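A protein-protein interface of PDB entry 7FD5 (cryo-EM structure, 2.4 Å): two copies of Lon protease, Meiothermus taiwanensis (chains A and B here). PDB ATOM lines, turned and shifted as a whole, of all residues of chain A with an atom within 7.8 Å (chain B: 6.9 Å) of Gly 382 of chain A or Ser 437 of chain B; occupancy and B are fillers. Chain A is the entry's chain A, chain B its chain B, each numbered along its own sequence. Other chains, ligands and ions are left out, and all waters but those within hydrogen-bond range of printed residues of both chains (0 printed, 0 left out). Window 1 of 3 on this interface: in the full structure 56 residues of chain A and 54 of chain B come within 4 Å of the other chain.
The side-chain carboxylate (OE2) of Glu 423 of chain A is in salt-bridge range of the side-chain amino group (NZ) of Lys 426 of chain A (2.8 Å). NH2 of Arg 391 of chain B lies within salt-bridge range of OE1 of Glu 441 of chain B, 2.8 Å away. OD2 of Asp 434 of chain B is in hydrogen-bond range of OG of Ser 437 of chain B, at 2.6 Å.
1 position is printed for both chains. Of the 5 pairs that touch across the chains among the printed residues, none has its exchanged pair printed and touching as well.
Of the 14 printed residues of chain B, 4 touch a printed residue of chain A. Of the 15 printed residues of chain A, 4 touch a printed residue of chain B.
Printed residues of chain B within 4 Å of Ser 380 of chain A: Arg 391 and Glu 441. Of chain B, only Ser 437 (3.1 Å) comes within 4 Å of Gly 382 of chain A. Printed residues of chain B within 4 Å of Lys 426 of chain A: Ser 437 (3.3 Å). Of the printed residues of chain A, Arg 391 of chain B touches Ser 380 (3.9 Å). No residue of chain A comes within 4 Å of Ala 436 of chain B. Of chain A, only Gly 382 (3.1 Å) and Lys 426 (3.3 Å) come within 4 Å of Ser 437 of chain B. Printed residues of chain A within 4 Å of Glu 441 of chain B: Ser 380 (3.6 Å).
Among the printed residues, pairs that only touch across the chains: Lys 426 of chain A with Ser 437 of chain B (3.3 Å), Ser 380 of chain A with Glu 441 of chain B (3.6 Å) and Ser 380 of chain A with Arg 391 of chain B (3.9 Å).
The backbone carbonyl oxygen (O) of Ser 437 of chain B sits close to the backbone carbonyl oxygen (O) of Gly 382 of chain A. OE2 of Glu 387 of chain B lies close to O of Gly 383 of chain A (3.1 Å).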
ATOM      1  N   ILE A 379       9.940 -37.000   9.931  1.00  0.00           N
ATOM      2  CA  ILE A 379       8.646 -36.350   9.880  1.00  0.00           C
ATOM      3  C   ILE A 379       8.862 -34.938   9.386  1.00  0.00           C
ATOM      4  O   ILE A 379       9.661 -34.190   9.951  1.00  0.00           O
ATOM      5  CB  ILE A 379       7.955 -36.357  11.245  1.00  0.00           C
ATOM      6  CG1 ILE A 379       7.618 -37.779  11.640  1.00  0.00           C
ATOM      7  CG2 ILE A 379       6.704 -35.570  11.187  1.00  0.00           C
ATOM      8  CD1 ILE A 379       7.157 -37.897  13.020  1.00  0.00           C
ATOM      9  N   SER A 380       8.169 -34.574   8.329  1.00  0.00           N
ATOM     10  CA  SER A 380       8.306 -33.247   7.760  1.00  0.00           C
ATOM     11  C   SER A 380       7.185 -32.392   8.314  1.00  0.00           C
ATOM     12  O   SER A 380       6.064 -32.398   7.820  1.00  0.00           O
ATOM     13  CB  SER A 380       8.274 -33.290   6.248  1.00  0.00           C
ATOM     14  OG  SER A 380       8.424 -31.983   5.750  1.00  0.00           O
ATOM     15  N   LEU A 381       7.507 -31.645   9.351  1.00  0.00           N
ATOM     16  CA  LEU A 381       6.654 -30.589   9.842  1.00  0.00           C
ATOM     17  C   LEU A 381       6.852 -29.370   8.971  1.00  0.00           C
ATOM     18  O   LEU A 381       7.404 -29.432   7.876  1.00  0.00           O
ATOM     19  CB  LEU A 381       6.999 -30.243  11.278  1.00  0.00           C
ATOM     20  CG  LEU A 381       6.876 -31.352  12.296  1.00  0.00           C
ATOM     21  CD1 LEU A 381       7.417 -30.821  13.573  1.00  0.00           C
ATOM     22  CD2 LEU A 381       5.447 -31.767  12.454  1.00  0.00           C
ATOM     23  N   GLY A 382       6.411 -28.238   9.451  1.00  0.00           N
ATOM     24  CA  GLY A 382       6.902 -27.066   8.788  1.00  0.00           C
ATOM     25  C   GLY A 382       6.012 -26.636   7.663  1.00  0.00           C
ATOM     26  O   GLY A 382       6.464 -26.004   6.721  1.00  0.00           O
ATOM     27  N   GLY A 383       4.776 -27.079   7.692  1.00  0.00           N
ATOM     28  CA  GLY A 383       3.720 -26.305   7.106  1.00  0.00           C
ATOM     29  C   GLY A 383       2.442 -26.581   7.848  1.00  0.00           C
ATOM     30  O   GLY A 383       1.372 -26.112   7.477  1.00  0.00           O
ATOM     31  N   VAL A 384       2.564 -27.342   8.926  1.00  0.00           N
ATOM     32  CA  VAL A 384       1.428 -28.043   9.492  1.00  0.00           C
ATOM     33  C   VAL A 384       0.612 -27.085  10.344  1.00  0.00           C
ATOM     34  O   VAL A 384       1.167 -26.255  11.067  1.00  0.00           O
ATOM     35  CB  VAL A 384       1.935 -29.244  10.294  1.00  0.00           C
ATOM     36  CG1 VAL A 384       0.819 -30.013  10.886  1.00  0.00           C
ATOM     37  CG2 VAL A 384       2.740 -30.114   9.405  1.00  0.00           C
ATOM     38  N   ARG A 385      -0.712 -27.162  10.224  1.00  0.00           N
ATOM     39  CA  ARG A 385      -1.627 -26.369  11.033  1.00  0.00           C
ATOM     40  C   ARG A 385      -2.428 -27.191  12.016  1.00  0.00           C
ATOM     41  O   ARG A 385      -2.626 -26.757  13.146  1.00  0.00           O
ATOM     42  CB  ARG A 385      -2.622 -25.625  10.158  1.00  0.00           C
ATOM     43  CG  ARG A 385      -2.072 -24.562   9.299  1.00  0.00           C
ATOM     44  CD  ARG A 385      -3.235 -23.974   8.564  1.00  0.00           C
ATOM     45  NE  ARG A 385      -3.892 -25.008   7.773  1.00  0.00           N
ATOM     46  CZ  ARG A 385      -5.053 -24.853   7.151  1.00  0.00           C
ATOM     47  NH1 ARG A 385      -5.697 -23.701   7.227  1.00  0.00           N
ATOM     48  NH2 ARG A 385      -5.571 -25.852   6.458  1.00  0.00           N
ATOM     49  N   LEU A 421      12.792 -34.351  13.237  1.00  0.00           N
ATOM     50  CA  LEU A 421      11.631 -33.476  13.107  1.00  0.00           C
ATOM     51  C   LEU A 421      12.040 -32.304  12.251  1.00  0.00           C
ATOM     52  O   LEU A 421      12.624 -31.342  12.735  1.00  0.00           O
ATOM     53  CB  LEU A 421      11.143 -32.993  14.459  1.00  0.00           C
ATOM     54  CG  LEU A 421      10.629 -34.059  15.391  1.00  0.00           C
ATOM     55  CD1 LEU A 421      10.205 -33.404  16.642  1.00  0.00           C
ATOM     56  CD2 LEU A 421       9.491 -34.761  14.753  1.00  0.00           C
ATOM     57  N   ASP A 422      11.706 -32.366  10.984  1.00  0.00           N
ATOM     58  CA  ASP A 422      12.336 -31.489  10.025  1.00  0.00           C
ATOM     59  C   ASP A 422      11.631 -30.146   9.996  1.00  0.00           C
ATOM     60  O   ASP A 422      10.408 -30.088   9.864  1.00  0.00           O
ATOM     61  CB  ASP A 422      12.307 -32.129   8.649  1.00  0.00           C
ATOM     62  CG  ASP A 422      13.406 -31.639   7.771  1.00  0.00           C
ATOM     63  OD1 ASP A 422      14.258 -30.890   8.270  1.00  0.00           O
ATOM     64  OD2 ASP A 422      13.419 -31.993   6.581  1.00  0.00           O
ATOM     65  N   GLU A 423      12.413 -29.077  10.121  1.00  0.00           N
ATOM     66  CA  GLU A 423      11.997 -27.693   9.903  1.00  0.00           C
ATOM     67  C   GLU A 423      10.901 -27.266  10.885  1.00  0.00           C
ATOM     68  O   GLU A 423       9.760 -27.042  10.519  1.00  0.00           O
ATOM     69  CB  GLU A 423      11.558 -27.501   8.448  1.00  0.00           C
ATOM     70  CG  GLU A 423      11.550 -26.082   7.983  1.00  0.00           C
ATOM     71  CD  GLU A 423      12.962 -25.510   7.833  1.00  0.00           C
ATOM     72  OE1 GLU A 423      13.901 -26.290   7.572  1.00  0.00           O
ATOM     73  OE2 GLU A 423      13.134 -24.274   7.972  1.00  0.00           O
ATOM     74  N   ILE A 424      11.280 -27.176  12.165  1.00  0.00           N
ATOM     75  CA  ILE A 424      10.334 -26.738  13.192  1.00  0.00           C
ATOM     76  C   ILE A 424      10.220 -25.234  13.336  1.00  0.00           C
ATOM     77  O   ILE A 424       9.509 -24.774  14.233  1.00  0.00           O
ATOM     78  CB  ILE A 424      10.650 -27.240  14.608  1.00  0.00           C
ATOM     79  CG1 ILE A 424      12.075 -26.900  14.966  1.00  0.00           C
ATOM     80  CG2 ILE A 424      10.372 -28.693  14.745  1.00  0.00           C
ATOM     81  CD1 ILE A 424      12.341 -27.143  16.376  1.00  0.00           C
ATOM     82  N   ASP A 425      10.932 -24.455  12.532  1.00  0.00           N
ATOM     83  CA  ASP A 425      10.576 -23.053  12.380  1.00  0.00           C
ATOM     84  C   ASP A 425       9.154 -22.909  11.888  1.00  0.00           C
ATOM     85  O   ASP A 425       8.349 -22.178  12.465  1.00  0.00           O
ATOM     86  CB  ASP A 425      11.479 -22.378  11.370  1.00  0.00           C
ATOM     87  CG  ASP A 425      12.824 -22.172  11.865  1.00  0.00           C
ATOM     88  OD1 ASP A 425      12.947 -22.015  13.086  1.00  0.00           O
ATOM     89  OD2 ASP A 425      13.755 -22.159  11.038  1.00  0.00           O
ATOM     90  N   LYS A 426       8.833 -23.607  10.812  1.00  0.00           N
ATOM     91  CA  LYS A 426       7.737 -23.236   9.950  1.00  0.00           C
ATOM     92  C   LYS A 426       6.430 -23.873  10.329  1.00  0.00           C
ATOM     93  O   LYS A 426       5.572 -24.022   9.462  1.00  0.00           O
ATOM     94  CB  LYS A 426       8.058 -23.595   8.511  1.00  0.00           C
ATOM     95  CG  LYS A 426       8.815 -22.561   7.744  1.00  0.00           C
ATOM     96  CD  LYS A 426      10.277 -22.638   7.943  1.00  0.00           C
ATOM     97  CE  LYS A 426      10.988 -21.724   6.974  1.00  0.00           C
ATOM     98  NZ  LYS A 426      12.451 -21.732   7.166  1.00  0.00           N
ATOM     99  N   MET A 427       6.255 -24.290  11.570  1.00  0.00           N
ATOM    100  CA  MET A 427       4.931 -24.701  11.986  1.00  0.00           C
ATOM    101  C   MET A 427       4.018 -23.495  12.014  1.00  0.00           C
ATOM    102  O   MET A 427       4.444 -22.381  12.314  1.00  0.00           O
ATOM    103  CB  MET A 427       4.954 -25.355  13.350  1.00  0.00           C
ATOM    104  CG  MET A 427       5.564 -26.704  13.348  1.00  0.00           C
ATOM    105  SD  MET A 427       5.217 -27.518  14.895  1.00  0.00           S
ATOM    106  CE  MET A 427       6.247 -26.534  15.954  1.00  0.00           C
ATOM    107  N   SER A 428       2.762 -23.717  11.673  1.00  0.00           N
ATOM    108  CA  SER A 428       1.809 -22.639  11.519  1.00  0.00           C
ATOM    109  C   SER A 428       0.631 -22.869  12.442  1.00  0.00           C
ATOM    110  O   SER A 428       0.187 -24.001  12.634  1.00  0.00           O
ATOM    111  CB  SER A 428       1.330 -22.538  10.083  1.00  0.00           C
ATOM    112  OG  SER A 428       0.426 -21.465   9.945  1.00  0.00           O
ATOM    113  N   GLU B 387      -3.137 -23.947   2.560  1.00  0.00           N
ATOM    114  CA  GLU B 387      -2.041 -24.884   2.516  1.00  0.00           C
ATOM    115  C   GLU B 387      -2.528 -26.306   2.370  1.00  0.00           C
ATOM    116  O   GLU B 387      -1.735 -27.214   2.147  1.00  0.00           O
ATOM    117  CB  GLU B 387      -1.216 -24.698   3.766  1.00  0.00           C
ATOM    118  CG  GLU B 387       0.130 -25.220   3.685  1.00  0.00           C
ATOM    119  CD  GLU B 387       0.973 -24.646   4.740  1.00  0.00           C
ATOM    120  OE1 GLU B 387       0.458 -23.852   5.563  1.00  0.00           O
ATOM    121  OE2 GLU B 387       2.168 -24.964   4.711  1.00  0.00           O
ATOM    122  N   ARG B 391      -0.559 -30.077   0.337  1.00  0.00           N
ATOM    123  CA  ARG B 391      -0.936 -31.350   0.919  1.00  0.00           C
ATOM    124  C   ARG B 391      -2.457 -31.422   0.903  1.00  0.00           C
ATOM    125  O   ARG B 391      -3.109 -30.615   0.254  1.00  0.00           O
ATOM    126  CB  ARG B 391      -0.349 -31.472   2.306  1.00  0.00           C
ATOM    127  CG  ARG B 391       1.144 -31.342   2.307  1.00  0.00           C
ATOM    128  CD  ARG B 391       1.693 -31.666   3.654  1.00  0.00           C
ATOM    129  NE  ARG B 391       3.144 -31.597   3.734  1.00  0.00           N
ATOM    130  CZ  ARG B 391       3.813 -30.565   4.223  1.00  0.00           C
ATOM    131  NH1 ARG B 391       3.164 -29.515   4.687  1.00  0.00           N
ATOM    132  NH2 ARG B 391       5.128 -30.589   4.262  1.00  0.00           N
ATOM    133  N   MET B 427       2.930 -16.390  -3.810  1.00  0.00           N
ATOM    134  CA  MET B 427       2.208 -17.181  -2.836  1.00  0.00           C
ATOM    135  C   MET B 427       2.068 -16.364  -1.570  1.00  0.00           C
ATOM    136  O   MET B 427       3.028 -15.739  -1.116  1.00  0.00           O
ATOM    137  CB  MET B 427       2.938 -18.477  -2.550  1.00  0.00           C
ATOM    138  CG  MET B 427       3.219 -19.232  -3.778  1.00  0.00           C
ATOM    139  SD  MET B 427       4.055 -20.769  -3.483  1.00  0.00           S
ATOM    140  CE  MET B 427       2.657 -21.753  -3.049  1.00  0.00           C
ATOM    141  N   SER B 429       2.362 -15.892   1.769  1.00  0.00           N
ATOM    142  CA  SER B 429       3.057 -16.538   2.873  1.00  0.00           C
ATOM    143  C   SER B 429       3.169 -15.535   4.011  1.00  0.00           C
ATOM    144  O   SER B 429       4.073 -14.694   4.015  1.00  0.00           O
ATOM    145  CB  SER B 429       4.431 -17.038   2.434  1.00  0.00           C
ATOM    146  OG  SER B 429       5.308 -15.966   2.141  1.00  0.00           O
ATOM    147  N   ASP B 434       1.292 -20.332   5.271  1.00  0.00           N
ATOM    148  CA  ASP B 434       2.236 -20.197   4.171  1.00  0.00           C
ATOM    149  C   ASP B 434       2.376 -21.495   3.400  1.00  0.00           C
ATOM    150  O   ASP B 434       2.984 -22.445   3.896  1.00  0.00           O
ATOM    151  CB  ASP B 434       3.594 -19.742   4.704  1.00  0.00           C
ATOM    152  CG  ASP B 434       4.007 -20.486   5.938  1.00  0.00           C
ATOM    153  OD1 ASP B 434       3.167 -21.230   6.477  1.00  0.00           O
ATOM    154  OD2 ASP B 434       5.171 -20.356   6.357  1.00  0.00           O
ATOM    155  N   PRO B 435       1.863 -21.583   2.177  1.00  0.00           N
ATOM    156  CA  PRO B 435       2.118 -22.771   1.366  1.00  0.00           C
ATOM    157  C   PRO B 435       3.539 -22.870   0.896  1.00  0.00           C
ATOM    158  O   PRO B 435       3.974 -23.959   0.519  1.00  0.00           O
ATOM    159  CB  PRO B 435       1.171 -22.590   0.187  1.00  0.00           C
ATOM    160  CG  PRO B 435       0.191 -21.653   0.642  1.00  0.00           C
ATOM    161  CD  PRO B 435       0.868 -20.719   1.547  1.00  0.00           C
ATOM    162  N   ALA B 436       4.280 -21.768   0.905  1.00  0.00           N
ATOM    163  CA  ALA B 436       5.670 -21.774   0.496  1.00  0.00           C
ATOM    164  C   ALA B 436       6.552 -22.559   1.443  1.00  0.00           C
ATOM    165  O   ALA B 436       7.667 -22.910   1.071  1.00  0.00           O
ATOM    166  CB  ALA B 436       6.184 -20.347   0.388  1.00  0.00           C
ATOM    167  N   SER B 437       6.089 -22.831   2.650  1.00  0.00           N
ATOM    168  CA  SER B 437       6.787 -23.720   3.551  1.00  0.00           C
ATOM    169  C   SER B 437       6.424 -25.171   3.332  1.00  0.00           C
ATOM    170  O   SER B 437       7.208 -26.046   3.682  1.00  0.00           O
ATOM    171  CB  SER B 437       6.478 -23.325   4.982  1.00  0.00           C
ATOM    172  OG  SER B 437       6.864 -21.993   5.196  1.00  0.00           O
ATOM    173  N   ALA B 438       5.267 -25.447   2.762  1.00  0.00           N
ATOM    174  CA  ALA B 438       4.967 -26.801   2.349  1.00  0.00           C
ATOM    175  C   ALA B 438       5.584 -27.142   1.010  1.00  0.00           C
ATOM    176  O   ALA B 438       5.739 -28.322   0.703  1.00  0.00           O
ATOM    177  CB  ALA B 438       3.464 -27.008   2.277  1.00  0.00           C
ATOM    178  N   MET B 439       5.943 -26.146   0.208  1.00  0.00           N
ATOM    179  CA  MET B 439       6.613 -26.423  -1.053  1.00  0.00           C
ATOM    180  C   MET B 439       8.050 -26.864  -0.881  1.00  0.00           C
ATOM    181  O   MET B 439       8.651 -27.306  -1.852  1.00  0.00           O
ATOM    182  CB  MET B 439       6.612 -25.208  -1.967  1.00  0.00           C
ATOM    183  CG  MET B 439       5.294 -24.837  -2.558  1.00  0.00           C
ATOM    184  SD  MET B 439       4.577 -26.130  -3.559  1.00  0.00           S
ATOM    185  CE  MET B 439       5.696 -26.163  -4.920  1.00  0.00           C
ATOM    186  N   LEU B 440       8.616 -26.756   0.313  1.00  0.00           N
ATOM    187  CA  LEU B 440       9.993 -27.168   0.520  1.00  0.00           C
ATOM    188  C   LEU B 440      10.160 -28.668   0.471  1.00  0.00           C
ATOM    189  O   LEU B 440      11.269 -29.142   0.241  1.00  0.00           O
ATOM    190  CB  LEU B 440      10.497 -26.680   1.858  1.00  0.00           C
ATOM    191  CG  LEU B 440      10.596 -25.187   2.043  1.00  0.00           C
ATOM    192  CD1 LEU B 440      10.933 -24.910   3.449  1.00  0.00           C
ATOM    193  CD2 LEU B 440      11.659 -24.675   1.164  1.00  0.00           C
ATOM    194  N   GLU B 441       9.102 -29.419   0.720  1.00  0.00           N
ATOM    195  CA  GLU B 441       9.150 -30.861   0.613  1.00  0.00           C
ATOM    196  C   GLU B 441       8.908 -31.330  -0.807  1.00  0.00           C
ATOM    197  O   GLU B 441       9.361 -32.410  -1.181  1.00  0.00           O
ATOM    198  CB  GLU B 441       8.112 -31.468   1.549  1.00  0.00           C
ATOM    199  CG  GLU B 441       8.260 -32.939   1.772  1.00  0.00           C
ATOM    200  CD  GLU B 441       7.175 -33.500   2.637  1.00  0.00           C
ATOM    201  OE1 GLU B 441       6.233 -32.758   2.964  1.00  0.00           O
ATOM    202  OE2 GLU B 441       7.275 -34.681   3.009  1.00  0.00           O
ATOM    203  N   PRO B 478      11.181 -17.027  -0.708  1.00  0.00           N
ATOM    204  CA  PRO B 478      11.978 -17.297   0.494  1.00  0.00           C
ATOM    205  C   PRO B 478      13.331 -17.911   0.183  1.00  0.00           C
ATOM    206  O   PRO B 478      13.492 -18.619  -0.805  1.00  0.00           O
ATOM    207  CB  PRO B 478      11.102 -18.274   1.272  1.00  0.00           C
ATOM    208  CG  PRO B 478       9.756 -17.975   0.832  1.00  0.00           C
ATOM    209  CD  PRO B 478       9.832 -17.586  -0.592  1.00  0.00           C
ATOM    210  N   LEU B 481      13.751 -21.730  -0.231  1.00  0.00           N
ATOM    211  CA  LEU B 481      13.061 -22.231  -1.409  1.00  0.00           C
ATOM    212  C   LEU B 481      13.770 -21.843  -2.689  1.00  0.00           C
ATOM    213  O   LEU B 481      13.709 -22.581  -3.668  1.00  0.00           O
ATOM    214  CB  LEU B 481      11.626 -21.723  -1.422  1.00  0.00           C
ATOM    215  CG  LEU B 481      10.720 -22.164  -2.558  1.00  0.00           C
ATOM    216  CD1 LEU B 481      10.639 -23.642  -2.580  1.00  0.00           C
ATOM    217  CD2 LEU B 481       9.360 -21.588  -2.396  1.00  0.00           C
